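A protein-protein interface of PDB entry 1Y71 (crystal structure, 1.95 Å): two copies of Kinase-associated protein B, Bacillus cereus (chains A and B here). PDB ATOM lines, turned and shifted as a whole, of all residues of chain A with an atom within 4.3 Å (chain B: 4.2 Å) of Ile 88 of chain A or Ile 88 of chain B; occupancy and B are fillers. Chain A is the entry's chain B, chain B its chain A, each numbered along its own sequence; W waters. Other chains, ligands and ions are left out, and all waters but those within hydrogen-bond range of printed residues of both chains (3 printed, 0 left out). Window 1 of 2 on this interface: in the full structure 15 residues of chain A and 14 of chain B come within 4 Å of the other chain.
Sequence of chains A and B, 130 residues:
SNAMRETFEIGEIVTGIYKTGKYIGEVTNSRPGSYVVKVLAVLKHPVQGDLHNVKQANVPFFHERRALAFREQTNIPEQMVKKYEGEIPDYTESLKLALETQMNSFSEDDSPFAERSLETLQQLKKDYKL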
ATOM      1  N   ILE A  13      22.133  -9.010  18.712  1.00  0.00           N
ATOM      2  CA  ILE A  13      21.065  -9.256  19.695  1.00  0.00           C
ATOM      3  C   ILE A  13      19.813  -9.773  18.994  1.00  0.00           C
ATOM      4  O   ILE A  13      19.340  -9.169  18.017  1.00  0.00           O
ATOM      5  CB  ILE A  13      20.733  -8.002  20.544  1.00  0.00           C
ATOM      6  CG1 ILE A  13      22.012  -7.442  21.173  1.00  0.00           C
ATOM      7  CG2 ILE A  13      19.709  -8.347  21.629  1.00  0.00           C
ATOM      8  CD1 ILE A  13      22.807  -8.501  21.997  1.00  0.00           C
ATOM      9  N   ILE A  24      15.701 -13.656  24.880  1.00  0.00           N
ATOM     10  CA  ILE A  24      16.567 -12.655  24.238  1.00  0.00           C
ATOM     11  C   ILE A  24      17.976 -13.130  24.470  1.00  0.00           C
ATOM     12  O   ILE A  24      18.333 -13.567  25.592  1.00  0.00           O
ATOM     13  CB  ILE A  24      16.336 -11.242  24.833  1.00  0.00           C
ATOM     14  CG1 ILE A  24      14.925 -10.792  24.466  1.00  0.00           C
ATOM     15  CG2 ILE A  24      17.478 -10.242  24.438  1.00  0.00           C
ATOM     16  CD1 ILE A  24      14.332  -9.716  25.369  1.00  0.00           C
ATOM     17  N   LEU A  40      20.390 -14.125  27.398  1.00  0.00           N
ATOM     18  CA  LEU A  40      20.497 -12.951  28.277  1.00  0.00           C
ATOM     19  C   LEU A  40      19.249 -12.644  29.106  1.00  0.00           C
ATOM     20  O   LEU A  40      19.338 -12.030  30.188  1.00  0.00           O
ATOM     21  CB  LEU A  40      20.883 -11.714  27.460  1.00  0.00           C
ATOM     22  CG  LEU A  40      22.203 -11.823  26.710  1.00  0.00           C
ATOM     23  CD1 LEU A  40      22.364 -10.635  25.727  1.00  0.00           C
ATOM     24  CD2 LEU A  40      23.459 -11.959  27.639  1.00  0.00           C
ATOM     25  N   PHE A  70      21.001 -18.060  32.594  1.00  0.00           N
ATOM     26  CA  PHE A  70      21.707 -16.858  32.181  1.00  0.00           C
ATOM     27  C   PHE A  70      23.066 -17.203  31.563  1.00  0.00           C
ATOM     28  O   PHE A  70      23.882 -17.936  32.151  1.00  0.00           O
ATOM     29  CB  PHE A  70      21.824 -15.834  33.361  1.00  0.00           C
ATOM     30  CG  PHE A  70      22.543 -14.587  32.980  1.00  0.00           C
ATOM     31  CD1 PHE A  70      22.065 -13.792  31.938  1.00  0.00           C
ATOM     32  CD2 PHE A  70      23.754 -14.247  33.591  1.00  0.00           C
ATOM     33  CE1 PHE A  70      22.753 -12.627  31.541  1.00  0.00           C
ATOM     34  CE2 PHE A  70      24.432 -13.096  33.202  1.00  0.00           C
ATOM     35  CZ  PHE A  70      23.938 -12.301  32.163  1.00  0.00           C
ATOM     36  N   GLY A  86      15.040  -4.244  20.942  1.00  0.00           N
ATOM     37  CA  GLY A  86      14.447  -3.663  22.158  1.00  0.00           C
ATOM     38  C   GLY A  86      15.491  -3.631  23.282  1.00  0.00           C
ATOM     39  O   GLY A  86      16.649  -4.052  23.081  1.00  0.00           O
ATOM     40  N   GLU A  87      15.070  -3.150  24.461  1.00  0.00           N
ATOM     41  CA  GLU A  87      15.935  -3.167  25.640  1.00  0.00           C
ATOM     42  C   GLU A  87      16.081  -4.586  26.117  1.00  0.00           C
ATOM     43  O   GLU A  87      15.203  -5.421  25.892  1.00  0.00           O
ATOM     44  CB  GLU A  87      15.408  -2.249  26.768  1.00  0.00           C
ATOM     45  CG  GLU A  87      15.438  -0.746  26.401  1.00  0.00           C
ATOM     46  CD  GLU A  87      15.040   0.141  27.549  1.00  0.00           C
ATOM     47  OE1 GLU A  87      14.752  -0.381  28.638  1.00  0.00           O
ATOM     48  OE2 GLU A  87      15.005   1.375  27.373  1.00  0.00           O
ATOM     49  N   ILE A  88      17.212  -4.864  26.750  1.00  0.00           N
ATOM     50  CA  ILE A  88      17.455  -6.184  27.291  1.00  0.00           C
ATOM     51  C   ILE A  88      17.109  -6.145  28.783  1.00  0.00           C
ATOM     52  O   ILE A  88      17.729  -5.404  29.557  1.00  0.00           O
ATOM     53  CB  ILE A  88      18.922  -6.654  27.059  1.00  0.00           C
ATOM     54  CG1 ILE A  88      19.253  -6.615  25.558  1.00  0.00           C
ATOM     55  CG2 ILE A  88      19.142  -8.073  27.681  1.00  0.00           C
ATOM     56  CD1 ILE A  88      20.673  -6.923  25.269  1.00  0.00           C
ATOM     57  N   PRO A  89      16.101  -6.916  29.190  1.00  0.00           N
ATOM     58  CA  PRO A  89      15.721  -6.922  30.590  1.00  0.00           C
ATOM     59  C   PRO A  89      16.758  -7.666  31.421  1.00  0.00           C
ATOM     60  O   PRO A  89      17.521  -8.451  30.880  1.00  0.00           O
ATOM     61  CB  PRO A  89      14.404  -7.710  30.619  1.00  0.00           C
ATOM     62  CG  PRO A  89      14.342  -8.455  29.378  1.00  0.00           C
ATOM     63  CD  PRO A  89      15.262  -7.803  28.364  1.00  0.00           C
ATOM     64  N   ASP A  90      16.758  -7.406  32.722  1.00  0.00           N
ATOM     65  CA  ASP A  90      17.552  -8.171  33.666  1.00  0.00           C
ATOM     66  C   ASP A  90      17.086  -9.617  33.648  1.00  0.00           C
ATOM     67  O   ASP A  90      15.866  -9.874  33.711  1.00  0.00           O
ATOM     68  CB  ASP A  90      17.353  -7.619  35.077  1.00  0.00           C
ATOM     69  CG  ASP A  90      18.097  -8.418  36.102  1.00  0.00           C
ATOM     70  OD1 ASP A  90      17.484  -9.227  36.861  1.00  0.00           O
ATOM     71  OD2 ASP A  90      19.313  -8.210  36.150  1.00  0.00           O
ATOM     72  N   ILE B  13      30.733  -8.979  26.136  1.00  0.00           N
ATOM     73  CA  ILE B  13      29.955  -8.137  27.052  1.00  0.00           C
ATOM     74  C   ILE B  13      30.942  -7.517  28.035  1.00  0.00           C
ATOM     75  O   ILE B  13      31.724  -8.238  28.667  1.00  0.00           O
ATOM     76  CB  ILE B  13      28.838  -8.923  27.780  1.00  0.00           C
ATOM     77  CG1 ILE B  13      27.886  -9.648  26.771  1.00  0.00           C
ATOM     78  CG2 ILE B  13      28.105  -8.011  28.803  1.00  0.00           C
ATOM     79  CD1 ILE B  13      27.118  -8.718  25.860  1.00  0.00           C
ATOM     80  N   ILE B  24      27.255  -0.712  30.752  1.00  0.00           N
ATOM     81  CA  ILE B  24      27.416  -2.068  30.333  1.00  0.00           C
ATOM     82  C   ILE B  24      27.115  -2.067  28.852  1.00  0.00           C
ATOM     83  O   ILE B  24      26.153  -1.442  28.425  1.00  0.00           O
ATOM     84  CB  ILE B  24      26.428  -3.012  31.078  1.00  0.00           C
ATOM     85  CG1 ILE B  24      26.831  -3.124  32.572  1.00  0.00           C
ATOM     86  CG2 ILE B  24      26.312  -4.377  30.323  1.00  0.00           C
ATOM     87  CD1 ILE B  24      25.740  -3.605  33.497  1.00  0.00           C
ATOM     88  N   LEU B  40      24.284  -0.993  26.368  1.00  0.00           N
ATOM     89  CA  LEU B  40      23.107  -1.787  26.727  1.00  0.00           C
ATOM     90  C   LEU B  40      22.450  -1.374  28.084  1.00  0.00           C
ATOM     91  O   LEU B  40      21.260  -1.608  28.296  1.00  0.00           O
ATOM     92  CB  LEU B  40      23.496  -3.276  26.789  1.00  0.00           C
ATOM     93  CG  LEU B  40      24.015  -3.797  25.442  1.00  0.00           C
ATOM     94  CD1 LEU B  40      24.458  -5.255  25.609  1.00  0.00           C
ATOM     95  CD2 LEU B  40      22.950  -3.588  24.268  1.00  0.00           C
ATOM     96  N   GLY B  86      28.166  -9.985  34.823  1.00  0.00           N
ATOM     97  CA  GLY B  86      26.880  -9.972  35.504  1.00  0.00           C
ATOM     98  C   GLY B  86      25.700  -9.948  34.537  1.00  0.00           C
ATOM     99  O   GLY B  86      25.864  -9.997  33.303  1.00  0.00           O
ATOM    100  N   GLU B  87      24.494  -9.852  35.099  1.00  0.00           N
ATOM    101  CA  GLU B  87      23.312  -9.770  34.273  1.00  0.00           C
ATOM    102  C   GLU B  87      23.250  -8.391  33.624  1.00  0.00           C
ATOM    103  O   GLU B  87      23.742  -7.395  34.169  1.00  0.00           O
ATOM    104  CB  GLU B  87      22.044 -10.018  35.102  1.00  0.00           C
ATOM    105  CG  GLU B  87      21.985 -11.346  35.818  1.00  0.00           C
ATOM    106  CD  GLU B  87      20.610 -11.572  36.448  1.00  0.00           C
ATOM    107  OE1 GLU B  87      19.873 -10.602  36.677  1.00  0.00           O
ATOM    108  OE2 GLU B  87      20.275 -12.706  36.764  1.00  0.00           O
ATOM    109  N   ILE B  88      22.627  -8.323  32.464  1.00  0.00           N
ATOM    110  CA  ILE B  88      22.424  -7.010  31.821  1.00  0.00           C
ATOM    111  C   ILE B  88      21.084  -6.423  32.306  1.00  0.00           C
ATOM    112  O   ILE B  88      20.040  -6.979  32.018  1.00  0.00           O
ATOM    113  CB  ILE B  88      22.475  -7.143  30.286  1.00  0.00           C
ATOM    114  CG1 ILE B  88      23.868  -7.689  29.859  1.00  0.00           C
ATOM    115  CG2 ILE B  88      22.095  -5.780  29.563  1.00  0.00           C
ATOM    116  CD1 ILE B  88      23.965  -8.041  28.326  1.00  0.00           C
ATOM    117  N   PRO B  89      21.113  -5.303  33.049  1.00  0.00           N
ATOM    118  CA  PRO B  89      19.853  -4.758  33.520  1.00  0.00           C
ATOM    119  C   PRO B  89      19.105  -4.080  32.376  1.00  0.00           C
ATOM    120  O   PRO B  89      19.702  -3.700  31.354  1.00  0.00           O
ATOM    121  CB  PRO B  89      20.277  -3.710  34.572  1.00  0.00           C
ATOM    122  CG  PRO B  89      21.647  -3.294  34.180  1.00  0.00           C
ATOM    123  CD  PRO B  89      22.266  -4.469  33.434  1.00  0.00           C
ATOM    124  N   ASP B  90      17.802  -3.917  32.538  1.00  0.00           N
ATOM    125  CA  ASP B  90      17.066  -3.134  31.559  1.00  0.00           C
ATOM    126  C   ASP B  90      17.597  -1.680  31.467  1.00  0.00           C
ATOM    127  O   ASP B  90      17.780  -0.999  32.486  1.00  0.00           O
ATOM    128  CB  ASP B  90      15.599  -3.127  31.881  1.00  0.00           C
ATOM    129  CG  ASP B  90      14.843  -2.201  30.984  1.00  0.00           C
ATOM    130  OD1 ASP B  90      14.578  -1.092  31.429  1.00  0.00           O
ATOM    131  OD2 ASP B  90      14.633  -2.538  29.801  1.00  0.00           O
HETATM  132  O   HOH W   1      20.398  -9.907  31.636  1.00  0.00           O
HETATM  133  O   HOH W   2      19.072  -9.936  39.560  1.00  0.00           O
HETATM  134  O   HOH W   3      18.946  -3.165  28.144  1.00  0.00           O
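The side-chain carboxylate (OE1) of Glu 87 of chain B sits close to the side-chain carboxylate (OD2) of Asp 90 of chain A, at 2.5 Å.
O of Ile 88 of chain B lies close to N of Asp 90 of chain A (3.4 Å).
The side-chain carboxylate of Glu 87 of chain A sits close to the side-chain carboxylate of Asp 90 of chain B (2.5 Å).
The backbone NH of Asp 90 of chain B sits close to the backbone carbonyl oxygen of Ile 88 of chain A (3.3 Å).
The backbone carbonyl oxygen of Ile 88 of chain A lies close to the backbone carbonyl oxygen of Pro 89 of chain B, at 3.2 Å.
The backbone carbonyl oxygen (O) of Pro 89 of chain A lies close to the backbone carbonyl oxygen (O) of Ile 88 of chain B, at 3.1 Å.
Among the printed residues, pairs that only touch across the chains: Phe 70 of chain A with Gly 86 of chain B, Phe 70 of chain A with Glu 87 of chain B, Asp 90 of chain A with Asp 90 of chain B and Ile 88 of chain A with Ile 88 of chain B.
Leu 40 of chain A touches none of the printed residues of chain B.
Ile 88 of chain A touches just these residues of chain B: Ile 88 (3.7 Å), Pro 89 (3.2 Å) and Asp 90 (3.1 Å).
Of the printed residues of chain B, Pro 89 of chain A touches Ile 88 (3.1 Å).
Of the printed residues of chain A, Gly 86 of chain B touches Phe 70 (3.2 Å).
Of the printed residues of chain A, Ile 88 of chain B touches Ile 88, Pro 89 and Asp 90.
The nearest printed residue of chain B that does not touch Ile 88 of chain A is Leu 40 of chain B (4.2 Å).
The nearest printed residue of chain A that does not touch Ile 88 of chain B is Leu 40 of chain A (4.01 Å).
The nearest printed residue of chain A that does not touch Glu 87 of chain B is Leu 40 of chain A (6.0 Å).
Along chain B the printed residues that touch a printed residue of chain A span positions 86 to 90.
Of the 9 printed residues of chain A, 5 touch a printed residue of chain B.
Among the printed residues, 10 pairs touch across the chains.
Among the printed residues, no Asp or Glu carboxylate lies within 4 Å of a Lys or Arg side-chain nitrogen of the other chain.
Glu 87 of chain A touches Asp 90 of chain B, and with the chains exchanged Asp 90 of chain A touches Glu 87 of chain B.
Ile 88 of chain A touches Pro 89 of chain B, and with the chains exchanged Pro 89 of chain A touches Ile 88 of chain B.
Ile 88 of chain A touches Asp 90 of chain B, and with the chains exchanged Asp 90 of chain A touches Ile 88 of chain B.
Asp 90 of chain A touches its own counterpart, Asp 90 of chain B.
Positions printed for both chains: 13, 24, 40, 86, 87, 88, 89 and 90.
Water W1 lies within hydrogen-bond range of O of Leu 40 of chain A (2.8 Å), N of Ile 88 of chain B (2.9 Å) and O of Pro 89 of chain A (3.3 Å).
Water W3 lies within hydrogen-bond range of the backbone carbonyl oxygen (O) of Leu 40 of chain B (2.8 Å), the backbone NH (N) of Ile 88 of chain A (2.8 Å) and the backbone carbonyl oxygen (O) of Pro 89 of chain B (3.3 Å).
Water W2 bridges the side-chain carboxylate of Glu 87 of chain B (3.1 Å) and the side-chain carboxylate of Asp 90 of chain A (3.2 Å).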
